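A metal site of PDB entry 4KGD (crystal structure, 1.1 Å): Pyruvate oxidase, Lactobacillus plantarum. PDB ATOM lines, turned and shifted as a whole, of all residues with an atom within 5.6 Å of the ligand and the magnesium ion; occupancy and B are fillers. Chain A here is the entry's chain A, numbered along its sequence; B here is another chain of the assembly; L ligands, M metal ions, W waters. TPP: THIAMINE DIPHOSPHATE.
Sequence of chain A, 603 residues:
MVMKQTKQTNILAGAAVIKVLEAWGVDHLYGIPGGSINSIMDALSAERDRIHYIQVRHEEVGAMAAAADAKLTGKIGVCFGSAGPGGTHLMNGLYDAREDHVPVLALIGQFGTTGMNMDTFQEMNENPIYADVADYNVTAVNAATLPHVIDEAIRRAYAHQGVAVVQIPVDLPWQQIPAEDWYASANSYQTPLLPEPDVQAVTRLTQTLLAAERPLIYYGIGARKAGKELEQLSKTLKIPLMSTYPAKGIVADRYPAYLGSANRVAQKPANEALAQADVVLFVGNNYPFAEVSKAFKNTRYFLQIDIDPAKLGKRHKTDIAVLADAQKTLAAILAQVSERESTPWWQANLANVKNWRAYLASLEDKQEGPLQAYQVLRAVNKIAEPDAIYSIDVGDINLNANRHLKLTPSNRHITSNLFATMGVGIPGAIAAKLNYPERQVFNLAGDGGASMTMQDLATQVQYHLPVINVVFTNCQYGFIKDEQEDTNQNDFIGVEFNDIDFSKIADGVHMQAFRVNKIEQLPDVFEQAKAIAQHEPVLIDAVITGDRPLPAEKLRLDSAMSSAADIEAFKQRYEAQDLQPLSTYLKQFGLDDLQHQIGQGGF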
ATOM      1  N   ASN A  92     -25.828  18.155 -17.236  1.00  0.00           N
ATOM      2  CA  ASN A  92     -25.367  17.348 -16.114  1.00  0.00           C
ATOM      3  C   ASN A  92     -25.650  18.042 -14.789  1.00  0.00           C
ATOM      4  O   ASN A  92     -25.876  17.378 -13.771  1.00  0.00           O
ATOM      5  CB  ASN A  92     -23.904  16.958 -16.221  1.00  0.00           C
ATOM      6  CG  ASN A  92     -23.770  15.795 -17.163  1.00  0.00           C
ATOM      7  OD1 ASN A  92     -24.330  15.783 -18.247  1.00  0.00           O
ATOM      8  ND2 ASN A  92     -23.056  14.760 -16.744  1.00  0.00           N
ATOM      9  N   ASP A 393     -15.933  15.179  -5.564  1.00  0.00           N
ATOM     10  CA  ASP A 393     -16.249  14.670  -6.894  1.00  0.00           C
ATOM     11  C   ASP A 393     -16.770  13.226  -6.741  1.00  0.00           C
ATOM     12  O   ASP A 393     -17.227  12.830  -5.679  1.00  0.00           O
ATOM     13  CB  ASP A 393     -15.035  14.833  -7.832  1.00  0.00           C
ATOM     14  CG  ASP A 393     -15.456  15.084  -9.275  1.00  0.00           C
ATOM     15  OD1 ASP A 393     -15.929  14.163  -9.950  1.00  0.00           O
ATOM     16  OD2 ASP A 393     -15.286  16.266  -9.713  1.00  0.00           O
ATOM     17  N   VAL A 394     -16.722  12.445  -7.845  1.00  0.00           N
ATOM     18  CA  VAL A 394     -17.391  11.133  -7.903  1.00  0.00           C
ATOM     19  C   VAL A 394     -16.363  10.082  -8.274  1.00  0.00           C
ATOM     20  O   VAL A 394     -15.672  10.200  -9.310  1.00  0.00           O
ATOM     21  CB  VAL A 394     -18.558  11.171  -8.902  1.00  0.00           C
ATOM     22  CG1 VAL A 394     -19.106   9.782  -9.206  1.00  0.00           C
ATOM     23  CG2 VAL A 394     -19.627  12.089  -8.366  1.00  0.00           C
ATOM     24  N   GLY A 395     -16.280   9.019  -7.461  1.00  0.00           N
ATOM     25  CA  GLY A 395     -15.360   7.925  -7.687  1.00  0.00           C
ATOM     26  C   GLY A 395     -14.845   7.387  -6.368  1.00  0.00           C
ATOM     27  O   GLY A 395     -15.520   7.488  -5.338  1.00  0.00           O
ATOM     28  N   ASP A 396     -13.622   6.844  -6.397  1.00  0.00           N
ATOM     29  CA  ASP A 396     -13.047   6.378  -5.158  1.00  0.00           C
ATOM     30  C   ASP A 396     -13.023   7.476  -4.084  1.00  0.00           C
ATOM     31  O   ASP A 396     -13.067   7.132  -2.901  1.00  0.00           O
ATOM     32  CB  ASP A 396     -11.651   5.848  -5.366  1.00  0.00           C
ATOM     33  CG  ASP A 396     -11.486   4.475  -5.917  1.00  0.00           C
ATOM     34  OD1 ASP A 396     -12.428   3.686  -5.893  1.00  0.00           O
ATOM     35  OD2 ASP A 396     -10.313   4.154  -6.301  1.00  0.00           O
ATOM     36  N   ILE A 397     -12.927   8.745  -4.442  1.00  0.00           N
ATOM     37  CA  ILE A 397     -12.931   9.771  -3.415  1.00  0.00           C
ATOM     38  C   ILE A 397     -14.158   9.726  -2.550  1.00  0.00           C
ATOM     39  O   ILE A 397     -14.051  10.059  -1.354  1.00  0.00           O
ATOM     40  CB  ILE A 397     -12.720  11.182  -4.021  1.00  0.00           C
ATOM     41  CG1 ILE A 397     -12.413  12.227  -2.958  1.00  0.00           C
ATOM     42  CG2 ILE A 397     -13.881  11.632  -4.910  1.00  0.00           C
ATOM     43  CD1 ILE A 397     -11.237  11.934  -2.059  1.00  0.00           C
ATOM     44  N   PHE A 419     -27.549  11.348  -8.973  1.00  0.00           N
ATOM     45  CA  PHE A 419     -27.155  11.357 -10.380  1.00  0.00           C
ATOM     46  C   PHE A 419     -25.668  10.979 -10.525  1.00  0.00           C
ATOM     47  O   PHE A 419     -25.237  10.419 -11.544  1.00  0.00           O
ATOM     48  CB  PHE A 419     -27.445  12.734 -10.984  1.00  0.00           C
ATOM     49  CG  PHE A 419     -27.363  12.781 -12.504  1.00  0.00           C
ATOM     50  CD1 PHE A 419     -28.178  11.994 -13.291  1.00  0.00           C
ATOM     51  CD2 PHE A 419     -26.490  13.685 -13.116  1.00  0.00           C
ATOM     52  CE1 PHE A 419     -28.121  12.100 -14.672  1.00  0.00           C
ATOM     53  CE2 PHE A 419     -26.437  13.762 -14.503  1.00  0.00           C
ATOM     54  CZ  PHE A 419     -27.248  12.978 -15.253  1.00  0.00           C
ATOM     55  N   ALA A 420     -24.876  11.329  -9.534  1.00  0.00           N
ATOM     56  CA  ALA A 420     -23.473  10.992  -9.421  1.00  0.00           C
ATOM     57  C   ALA A 420     -22.705  11.409 -10.686  1.00  0.00           C
ATOM     58  O   ALA A 420     -21.891  10.665 -11.220  1.00  0.00           O
ATOM     59  CB  ALA A 420     -23.256   9.512  -9.107  1.00  0.00           C
ATOM     60  N   THR A 421     -22.890  12.668 -11.089  1.00  0.00           N
ATOM     61  CA  THR A 421     -22.087  13.203 -12.160  1.00  0.00           C
ATOM     62  C   THR A 421     -20.664  13.541 -11.687  1.00  0.00           C
ATOM     63  O   THR A 421     -20.462  14.344 -10.793  1.00  0.00           O
ATOM     64  CB  THR A 421     -22.742  14.390 -12.877  1.00  0.00           C
ATOM     65  OG1 THR A 421     -21.886  14.785 -13.961  1.00  0.00           O
ATOM     66  CG2 THR A 421     -23.025  15.569 -11.993  1.00  0.00           C
ATOM     67  N   MET A 422     -19.668  12.931 -12.368  1.00  0.00           N
ATOM     68  CA  MET A 422     -18.316  13.381 -12.231  1.00  0.00           C
ATOM     69  C   MET A 422     -18.200  14.842 -12.650  1.00  0.00           C
ATOM     70  O   MET A 422     -19.008  15.330 -13.464  1.00  0.00           O
ATOM     71  CB  MET A 422     -17.396  12.547 -13.096  1.00  0.00           C
ATOM     72  CG  MET A 422     -17.215  11.090 -12.659  1.00  0.00           C
ATOM     73  SD  MET A 422     -16.489  10.072 -13.912  1.00  0.00           S
ATOM     74  CE  MET A 422     -14.870  10.803 -14.056  1.00  0.00           C
ATOM     75  N   ALA A 445     -11.088  15.607  -5.499  1.00  0.00           N
ATOM     76  CA  ALA A 445     -11.486  15.030  -6.810  1.00  0.00           C
ATOM     77  C   ALA A 445     -10.468  14.016  -7.283  1.00  0.00           C
ATOM     78  O   ALA A 445      -9.261  14.198  -7.173  1.00  0.00           O
ATOM     79  CB  ALA A 445     -11.601  16.129  -7.845  1.00  0.00           C
ATOM     80  N   GLY A 446     -10.981  12.942  -7.892  1.00  0.00           N
ATOM     81  CA  GLY A 446     -10.132  12.084  -8.676  1.00  0.00           C
ATOM     82  C   GLY A 446      -9.659  12.736  -9.970  1.00  0.00           C
ATOM     83  O   GLY A 446     -10.230  13.742 -10.399  1.00  0.00           O
ATOM     84  N   ASP A 447      -8.659  12.144 -10.574  1.00  0.00           N
ATOM     85  CA  ASP A 447      -8.111  12.695 -11.813  1.00  0.00           C
ATOM     86  C   ASP A 447      -9.118  12.642 -12.961  1.00  0.00           C
ATOM     87  O   ASP A 447      -9.179  13.565 -13.784  1.00  0.00           O
ATOM     88  CB  ASP A 447      -6.796  12.056 -12.197  1.00  0.00           C
ATOM     89  CG  ASP A 447      -6.662  10.533 -12.194  1.00  0.00           C
ATOM     90  OD1 ASP A 447      -7.631   9.821 -11.868  1.00  0.00           O
ATOM     91  OD2 ASP A 447      -5.551  10.071 -12.526  1.00  0.00           O
ATOM     92  N   GLY A 448      -9.921  11.590 -13.051  1.00  0.00           N
ATOM     93  CA  GLY A 448     -10.924  11.528 -14.092  1.00  0.00           C
ATOM     94  C   GLY A 448     -11.971  12.614 -13.964  1.00  0.00           C
ATOM     95  O   GLY A 448     -12.305  13.297 -14.948  1.00  0.00           O
ATOM     96  N   GLY A 449     -12.459  12.855 -12.745  1.00  0.00           N
ATOM     97  CA  GLY A 449     -13.476  13.866 -12.518  1.00  0.00           C
ATOM     98  C   GLY A 449     -12.933  15.270 -12.626  1.00  0.00           C
ATOM     99  O   GLY A 449     -13.552  16.162 -13.243  1.00  0.00           O
ATOM    100  N   ALA A 450     -11.765  15.508 -12.052  1.00  0.00           N
ATOM    101  CA  ALA A 450     -11.104  16.811 -12.179  1.00  0.00           C
ATOM    102  C   ALA A 450     -10.876  17.141 -13.632  1.00  0.00           C
ATOM    103  O   ALA A 450     -11.007  18.295 -14.034  1.00  0.00           O
ATOM    104  CB  ALA A 450      -9.796  16.841 -11.432  1.00  0.00           C
ATOM    105  N   MET A 452     -12.623  16.391 -16.180  1.00  0.00           N
ATOM    106  CA  MET A 452     -13.843  16.773 -16.879  1.00  0.00           C
ATOM    107  C   MET A 452     -14.165  18.233 -16.737  1.00  0.00           C
ATOM    108  O   MET A 452     -14.767  18.785 -17.680  1.00  0.00           O
ATOM    109  CB  MET A 452     -15.052  15.914 -16.417  1.00  0.00           C
ATOM    110  CG  MET A 452     -14.930  14.492 -16.961  1.00  0.00           C
ATOM    111  SD  MET A 452     -16.340  13.526 -16.465  1.00  0.00           S
ATOM    112  CE  MET A 452     -15.962  12.009 -17.351  1.00  0.00           C
ATOM    113  N   PHE A 472      -6.547  13.459  -6.868  1.00  0.00           N
ATOM    114  CA  PHE A 472      -6.070  12.117  -6.553  1.00  0.00           C
ATOM    115  C   PHE A 472      -5.707  11.434  -7.874  1.00  0.00           C
ATOM    116  O   PHE A 472      -6.563  10.900  -8.559  1.00  0.00           O
ATOM    117  CB  PHE A 472      -7.089  11.308  -5.752  1.00  0.00           C
ATOM    118  CG  PHE A 472      -7.335  11.876  -4.366  1.00  0.00           C
ATOM    119  CD1 PHE A 472      -7.953  13.083  -4.108  1.00  0.00           C
ATOM    120  CD2 PHE A 472      -6.879  11.150  -3.251  1.00  0.00           C
ATOM    121  CE1 PHE A 472      -8.121  13.589  -2.855  1.00  0.00           C
ATOM    122  CE2 PHE A 472      -7.093  11.621  -1.988  1.00  0.00           C
ATOM    123  CZ  PHE A 472      -7.679  12.848  -1.759  1.00  0.00           C
ATOM    124  N   THR A 473      -4.424  11.498  -8.234  1.00  0.00           N
ATOM    125  CA  THR A 473      -3.980  11.011  -9.550  1.00  0.00           C
ATOM    126  C   THR A 473      -3.519   9.591  -9.463  1.00  0.00           C
ATOM    127  O   THR A 473      -2.398   9.318  -8.995  1.00  0.00           O
ATOM    128  CB  THR A 473      -2.923  11.958 -10.145  1.00  0.00           C
ATOM    129  OG1 THR A 473      -3.590  13.172 -10.459  1.00  0.00           O
ATOM    130  CG2 THR A 473      -2.318  11.343 -11.385  1.00  0.00           C
ATOM    131  N   ASN A 474      -4.394   8.658  -9.894  1.00  0.00           N
ATOM    132  CA  ASN A 474      -4.051   7.254  -9.993  1.00  0.00           C
ATOM    133  C   ASN A 474      -3.883   6.819 -11.457  1.00  0.00           C
ATOM    134  O   ASN A 474      -3.559   5.654 -11.686  1.00  0.00           O
ATOM    135  CB  ASN A 474      -5.034   6.350  -9.278  1.00  0.00           C
ATOM    136  CG  ASN A 474      -6.462   6.635  -9.602  1.00  0.00           C
ATOM    137  OD1 ASN A 474      -6.801   7.286 -10.578  1.00  0.00           O
ATOM    138  ND2 ASN A 474      -7.376   6.093  -8.786  1.00  0.00           N
ATOM    139  N   CYS A 475      -4.100   7.712 -12.422  1.00  0.00           N
ATOM    140  CA  CYS A 475      -4.085   7.329 -13.845  1.00  0.00           C
ATOM    141  C   CYS A 475      -5.079   6.239 -14.170  1.00  0.00           C
ATOM    142  O   CYS A 475      -4.898   5.432 -15.052  1.00  0.00           O
ATOM    143  CB  CYS A 475      -2.691   6.967 -14.318  1.00  0.00           C
ATOM    144  SG  CYS A 475      -1.500   8.318 -14.207  1.00  0.00           S
ATOM    145  N   GLN A 476      -6.212   6.307 -13.452  1.00  0.00           N
ATOM    146  CA  GLN A 476      -7.264   5.318 -13.627  1.00  0.00           C
ATOM    147  C   GLN A 476      -8.623   5.939 -13.382  1.00  0.00           C
ATOM    148  O   GLN A 476      -8.751   6.945 -12.644  1.00  0.00           O
ATOM    149  CB  GLN A 476      -7.163   4.169 -12.625  1.00  0.00           C
ATOM    150  CG  GLN A 476      -5.852   3.428 -12.616  1.00  0.00           C
ATOM    151  CD  GLN A 476      -5.740   2.417 -11.492  1.00  0.00           C
ATOM    152  OE1 GLN A 476      -5.016   1.393 -11.628  1.00  0.00           O
ATOM    153  NE2 GLN A 476      -6.389   2.581 -10.447  1.00  0.00           N
ATOM    154  N   TYR A 477      -9.626   5.304 -13.932  1.00  0.00           N
ATOM    155  CA  TYR A 477     -10.998   5.383 -13.410  1.00  0.00           C
ATOM    156  C   TYR A 477     -11.072   4.278 -12.357  1.00  0.00           C
ATOM    157  O   TYR A 477     -11.566   3.158 -12.652  1.00  0.00           O
ATOM    158  CB  TYR A 477     -12.038   5.203 -14.507  1.00  0.00           C
ATOM    159  CG  TYR A 477     -12.055   6.291 -15.554  1.00  0.00           C
ATOM    160  CD1 TYR A 477     -12.144   7.630 -15.218  1.00  0.00           C
ATOM    161  CD2 TYR A 477     -11.994   5.955 -16.882  1.00  0.00           C
ATOM    162  CE1 TYR A 477     -12.162   8.618 -16.196  1.00  0.00           C
ATOM    163  CE2 TYR A 477     -11.992   6.948 -17.857  1.00  0.00           C
ATOM    164  CZ  TYR A 477     -12.091   8.276 -17.517  1.00  0.00           C
ATOM    165  OH  TYR A 477     -12.071   9.228 -18.484  1.00  0.00           O
ATOM    166  N   GLY A 478     -10.499   4.493 -11.182  1.00  0.00           N
ATOM    167  CA  GLY A 478     -10.304   3.427 -10.231  1.00  0.00           C
ATOM    168  C   GLY A 478     -11.564   2.740  -9.815  1.00  0.00           C
ATOM    169  O   GLY A 478     -11.681   1.523  -9.762  1.00  0.00           O
ATOM    170  N   PHE A 479     -12.603   3.583  -9.544  1.00  0.00           N
ATOM    171  CA  PHE A 479     -13.892   3.029  -9.127  1.00  0.00           C
ATOM    172  C   PHE A 479     -14.423   2.016 -10.133  1.00  0.00           C
ATOM    173  O   PHE A 479     -15.037   1.023  -9.766  1.00  0.00           O
ATOM    174  CB  PHE A 479     -14.882   4.175  -8.922  1.00  0.00           C
ATOM    175  CG  PHE A 479     -15.999   4.005  -7.936  1.00  0.00           C
ATOM    176  CD1 PHE A 479     -15.742   3.904  -6.573  1.00  0.00           C
ATOM    177  CD2 PHE A 479     -17.291   3.996  -8.380  1.00  0.00           C
ATOM    178  CE1 PHE A 479     -16.832   3.787  -5.690  1.00  0.00           C
ATOM    179  CE2 PHE A 479     -18.348   3.890  -7.519  1.00  0.00           C
ATOM    180  CZ  PHE A 479     -18.106   3.809  -6.160  1.00  0.00           C
ATOM    181  N   ILE A 480     -14.232   2.330 -11.412  1.00  0.00           N
ATOM    182  CA  ILE A 480     -14.708   1.454 -12.494  1.00  0.00           C
ATOM    183  C   ILE A 480     -13.765   0.292 -12.766  1.00  0.00           C
ATOM    184  O   ILE A 480     -14.262  -0.814 -13.060  1.00  0.00           O
ATOM    185  CB  ILE A 480     -14.932   2.259 -13.789  1.00  0.00           C
ATOM    186  CG1 ILE A 480     -15.793   3.488 -13.536  1.00  0.00           C
ATOM    187  CG2 ILE A 480     -15.538   1.366 -14.875  1.00  0.00           C
ATOM    188  CD1 ILE A 480     -17.067   3.206 -12.825  1.00  0.00           C
ATOM    189  N   PHE A 497      -5.213   4.940 -17.932  1.00  0.00           N
ATOM    190  CA  PHE A 497      -4.959   5.958 -18.958  1.00  0.00           C
ATOM    191  C   PHE A 497      -3.691   6.730 -18.616  1.00  0.00           C
ATOM    192  O   PHE A 497      -3.041   6.507 -17.582  1.00  0.00           O
ATOM    193  CB  PHE A 497      -6.197   6.859 -19.115  1.00  0.00           C
ATOM    194  CG  PHE A 497      -6.791   7.425 -17.876  1.00  0.00           C
ATOM    195  CD1 PHE A 497      -6.085   8.349 -17.053  1.00  0.00           C
ATOM    196  CD2 PHE A 497      -8.060   7.068 -17.461  1.00  0.00           C
ATOM    197  CE1 PHE A 497      -6.709   8.870 -15.943  1.00  0.00           C
ATOM    198  CE2 PHE A 497      -8.677   7.596 -16.341  1.00  0.00           C
ATOM    199  CZ  PHE A 497      -7.984   8.473 -15.566  1.00  0.00           C
ATOM    200  N   ILE B  32     -16.530   6.378 -22.281  1.00  0.00           N
ATOM    201  CA  ILE B  32     -15.931   6.223 -20.971  1.00  0.00           C
ATOM    202  C   ILE B  32     -16.709   5.117 -20.291  1.00  0.00           C
ATOM    203  O   ILE B  32     -17.943   5.126 -20.303  1.00  0.00           O
ATOM    204  CB  ILE B  32     -16.023   7.545 -20.174  1.00  0.00           C
ATOM    205  CG1 ILE B  32     -15.075   8.578 -20.788  1.00  0.00           C
ATOM    206  CG2 ILE B  32     -15.726   7.353 -18.685  1.00  0.00           C
ATOM    207  CD1 ILE B  32     -15.168   9.980 -20.208  1.00  0.00           C
ATOM    208  N   PRO B  33     -16.014   4.138 -19.704  1.00  0.00           N
ATOM    209  CA  PRO B  33     -16.741   2.998 -19.097  1.00  0.00           C
ATOM    210  C   PRO B  33     -17.419   3.421 -17.787  1.00  0.00           C
ATOM    211  O   PRO B  33     -17.138   4.406 -17.167  1.00  0.00           O
ATOM    212  CB  PRO B  33     -15.626   1.988 -18.867  1.00  0.00           C
ATOM    213  CG  PRO B  33     -14.447   2.854 -18.555  1.00  0.00           C
ATOM    214  CD  PRO B  33     -14.564   4.017 -19.534  1.00  0.00           C
ATOM    215  N   GLY B  34     -18.328   2.555 -17.375  1.00  0.00           N
ATOM    216  CA  GLY B  34     -19.024   2.621 -16.115  1.00  0.00           C
ATOM    217  C   GLY B  34     -19.639   1.265 -15.826  1.00  0.00           C
ATOM    218  O   GLY B  34     -19.802   0.447 -16.747  1.00  0.00           O
ATOM    219  N   GLU B  59     -17.279  12.582 -22.164  1.00  0.00           N
ATOM    220  CA  GLU B  59     -18.119  11.934 -23.167  1.00  0.00           C
ATOM    221  C   GLU B  59     -18.609  12.866 -24.283  1.00  0.00           C
ATOM    222  O   GLU B  59     -18.887  12.380 -25.379  1.00  0.00           O
ATOM    223  CB  GLU B  59     -19.332  11.246 -22.534  1.00  0.00           C
ATOM    224  CG  GLU B  59     -18.983  10.176 -21.507  1.00  0.00           C
ATOM    225  CD  GLU B  59     -18.817  10.677 -20.082  1.00  0.00           C
ATOM    226  OE1 GLU B  59     -18.655  11.894 -19.846  1.00  0.00           O
ATOM    227  OE2 GLU B  59     -18.804   9.783 -19.194  1.00  0.00           O
ATOM    228  N   SER B  82     -22.087   6.036 -20.104  1.00  0.00           N
ATOM    229  CA  SER B  82     -22.648   5.311 -18.989  1.00  0.00           C
ATOM    230  C   SER B  82     -23.973   5.944 -18.541  1.00  0.00           C
ATOM    231  O   SER B  82     -24.324   7.113 -18.823  1.00  0.00           O
ATOM    232  CB  SER B  82     -21.598   5.326 -17.864  1.00  0.00           C
ATOM    233  OG  SER B  82     -21.281   6.675 -17.430  1.00  0.00           O
ATOM    234  N   PRO B  85     -25.222  10.461 -16.072  1.00  0.00           N
ATOM    235  CA  PRO B  85     -24.341  11.524 -16.514  1.00  0.00           C
ATOM    236  C   PRO B  85     -23.430  11.199 -17.666  1.00  0.00           C
ATOM    237  O   PRO B  85     -22.921  12.130 -18.313  1.00  0.00           O
ATOM    238  CB  PRO B  85     -23.518  11.841 -15.229  1.00  0.00           C
ATOM    239  CG  PRO B  85     -23.584  10.567 -14.433  1.00  0.00           C
ATOM    240  CD  PRO B  85     -25.000  10.092 -14.649  1.00  0.00           C
ATOM    241  N   GLY B  86     -23.061   9.952 -17.876  1.00  0.00           N
ATOM    242  CA  GLY B  86     -22.242   9.638 -19.052  1.00  0.00           C
ATOM    243  C   GLY B  86     -23.003   9.992 -20.337  1.00  0.00           C
ATOM    244  O   GLY B  86     -22.491  10.668 -21.222  1.00  0.00           O
ATOM    245  N   HIS B  89     -23.786  13.724 -20.938  1.00  0.00           N
ATOM    246  CA  HIS B  89     -22.620  14.407 -21.469  1.00  0.00           C
ATOM    247  C   HIS B  89     -22.503  14.310 -23.004  1.00  0.00           C
ATOM    248  O   HIS B  89     -21.771  15.115 -23.582  1.00  0.00           O
ATOM    249  CB  HIS B  89     -21.355  13.905 -20.824  1.00  0.00           C
ATOM    250  CG  HIS B  89     -20.873  14.670 -19.640  1.00  0.00           C
ATOM    251  ND1 HIS B  89     -19.776  14.261 -18.911  1.00  0.00           N
ATOM    252  CD2 HIS B  89     -21.184  15.898 -19.136  1.00  0.00           C
ATOM    253  CE1 HIS B  89     -19.488  15.179 -18.006  1.00  0.00           C
ATOM    254  NE2 HIS B  89     -20.335  16.188 -18.099  1.00  0.00           N
ATOM    255  N   GLN B 122     -28.222   5.853  -9.563  1.00  0.00           N
ATOM    256  CA  GLN B 122     -28.024   6.414 -10.895  1.00  0.00           C
ATOM    257  C   GLN B 122     -28.987   5.739 -11.868  1.00  0.00           C
ATOM    258  O   GLN B 122     -28.746   5.670 -13.070  1.00  0.00           O
ATOM    259  CB  GLN B 122     -26.562   6.408 -11.188  1.00  0.00           C
ATOM    260  CG  GLN B 122     -26.223   7.297 -12.423  1.00  0.00           C
ATOM    261  CD  GLN B 122     -24.737   7.037 -12.473  1.00  0.00           C
ATOM    262  OE1 GLN B 122     -23.997   7.974 -12.224  1.00  0.00           O
ATOM    263  NE2 GLN B 122     -24.477   5.833 -12.884  1.00  0.00           N
HETATM  264  N1' TPP L   1     -19.301   9.712 -16.614  1.00  0.00           N
HETATM  265  C2' TPP L   1     -19.723  10.686 -15.811  1.00  0.00           C
HETATM  266  CM2 TPP L   1     -19.802  12.055 -16.367  1.00  0.00           C
HETATM  267  N3' TPP L   1     -20.115  10.450 -14.549  1.00  0.00           N
HETATM  268  C4' TPP L   1     -20.039   9.151 -14.066  1.00  0.00           C
HETATM  269  N4' TPP L   1     -20.522   8.926 -12.828  1.00  0.00           N
HETATM  270  C5' TPP L   1     -19.458   8.138 -14.842  1.00  0.00           C
HETATM  271  C6' TPP L   1     -19.139   8.397 -16.131  1.00  0.00           C
HETATM  272  C7' TPP L   1     -19.177   6.744 -14.279  1.00  0.00           C
HETATM  273  N3  TPP L   1     -18.103   6.759 -13.296  1.00  0.00           N
HETATM  274  C2  TPP L   1     -18.444   6.661 -11.900  1.00  0.00           C
HETATM  275  S1  TPP L   1     -16.958   6.743 -10.982  1.00  0.00           S
HETATM  276  C5  TPP L   1     -15.997   6.771 -12.458  1.00  0.00           C
HETATM  277  C4  TPP L   1     -16.735   6.751 -13.580  1.00  0.00           C
HETATM  278  CM4 TPP L   1     -16.245   6.757 -15.005  1.00  0.00           C
HETATM  279  C6  TPP L   1     -14.514   6.839 -12.357  1.00  0.00           C
HETATM  280  C7  TPP L   1     -14.063   8.116 -11.644  1.00  0.00           C
HETATM  281  O7  TPP L   1     -12.603   8.212 -11.932  1.00  0.00           O
HETATM  282  PA  TPP L   1     -11.711   9.232 -11.104  1.00  0.00           P
HETATM  283  O1A TPP L   1     -10.333   9.172 -11.687  1.00  0.00           O
HETATM  284  O2A TPP L   1     -12.328  10.590 -11.049  1.00  0.00           O
HETATM  285  O3A TPP L   1     -11.736   8.633  -9.641  1.00  0.00           O
HETATM  286  PB  TPP L   1     -10.971   7.330  -8.998  1.00  0.00           P
HETATM  287  O1B TPP L   1      -9.904   6.930  -9.999  1.00  0.00           O
HETATM  288  O2B TPP L   1     -12.021   6.306  -8.773  1.00  0.00           O
HETATM  289  O3B TPP L   1     -10.363   7.919  -7.716  1.00  0.00           O
HETATM  290 MG    MG M   1      -8.645   8.233 -11.073  1.00  0.00          MG
HETATM  291  O   HOH W   1     -20.330   5.587  -9.381  1.00  0.00           O
HETATM  292  O   HOH W   2     -22.592   6.915 -15.097  1.00  0.00           O
HETATM  293  O   HOH W   3      -8.615   7.950  -5.592  1.00  0.00           O
HETATM  294  O   HOH W   4     -21.569   6.669 -11.413  1.00  0.00           O
HETATM  295  O   HOH W   5      -8.490   9.224  -9.234  1.00  0.00           O
HETATM  296  O   HOH W   6     -13.368  11.675  -8.829  1.00  0.00           O
HETATM  297  O   HOH W   7     -12.154   9.838  -6.904  1.00  0.00           O
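The side-chain carboxylate (OE2) of Glu 59 of chain B lies within hydrogen-bond range of a nitrogen (N1') of the ligand (2.6 Å). O of Ala 420 sits at hydrogen-bond distance from N4' of the ligand (2.7 Å). O2B of the ligand sits at hydrogen-bond distance from N of Gly 478. An oxygen (O2A) of the ligand lies within hydrogen-bond range of the backbone NH of Gly 448, at 3.3 Å. The backbone NH (N) of Gly 449 lies within hydrogen-bond range of an oxygen (O2A) of the ligand, at 2.8 Å. The backbone NH (N) of Phe 479 lies within hydrogen-bond range of an oxygen (O2B) of the ligand (2.9 Å). The backbone NH of Asp 396 sits at hydrogen-bond distance from an oxygen (O2B) of the ligand (2.9 Å). A nitrogen (N3') of the ligand lies within hydrogen-bond range of the backbone NH (N) of Met 422, 3.3 Å away.
The backbone NH of Asp 447 is in hydrogen-bond range of the backbone carbonyl oxygen of Phe 472, at 3.2 Å. The side-chain carboxylate (OD2) of Asp 447 sits at hydrogen-bond distance from the backbone NH (N) of Cys 475 (2.8 Å). The side-chain carboxylate (OE1) of Glu 59 of chain B lies within hydrogen-bond range of a ring nitrogen (ND1) of His 89 of chain B (2.8 Å). The side-chain amide nitrogen of Asn 92 lies close to a ring nitrogen (NE2) of His 89 of chain B (3.4 Å). O of Pro 85 of chain B is in hydrogen-bond range of ND2 of Asn 92. The side-chain amide oxygen (OE1) of Gln 122 of chain B lies close to the backbone carbonyl oxygen (O) of Phe 419 (2.8 Å).
Merely in contact with the ligand: Val 394, Gly 395, Gly 446, Met 452, Tyr 477, Ile 480, Ile 32 of chain B, Pro 33 of chain B, Ser 82 of chain B, Pro 85 of chain B, Gly 86 of chain B, His 89 of chain B and Gln 122 of chain B. Hydrophobic or aromatic side chains within 4 Å of the ligand: Val 394, Met 422, Met 452, Tyr 477, Phe 479, Ile 480, Ile 32 of chain B, Pro 85 of chain B and His 89 of chain B.
The magnesium ion is bound by an oxygen (O1A) of the ligand (2.0 Å). The backbone carbonyl oxygen (O) of Gln 476 is bound to the magnesium ion. OD1 of Asp 447 binds the magnesium ion (2.0 Å). Water W5 binds the magnesium ion (2.1 Å). An oxygen (O1B) of the ligand is bound to the magnesium ion (2.1 Å). The magnesium ion is bound by OD1 of Asn 474 (2.1 Å). The magnesium ion has six donor atoms within binding distance.
Water W5 lies within hydrogen-bond range of the backbone carbonyl oxygen of Phe 472 (2.6 Å), an oxygen (O3B) of the ligand (2.7 Å), the backbone NH of Asp 447 (3.2 Å) and the side-chain amide nitrogen of Asn 474 (3.4 Å). Water W6 lies within hydrogen-bond range of an oxygen (O2A) of the ligand (2.7 Å), the backbone carbonyl oxygen of Val 394 (2.8 Å) and the backbone NH of Gly 446 (2.9 Å). Water W4 lies within hydrogen-bond range of N4' of the ligand and OE1 of Gln 122 of chain B. Water W2 bridges OG of Ser 82 of chain B (2.7 Å) and NE2 of Gln 122 of chain B (3.1 Å).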
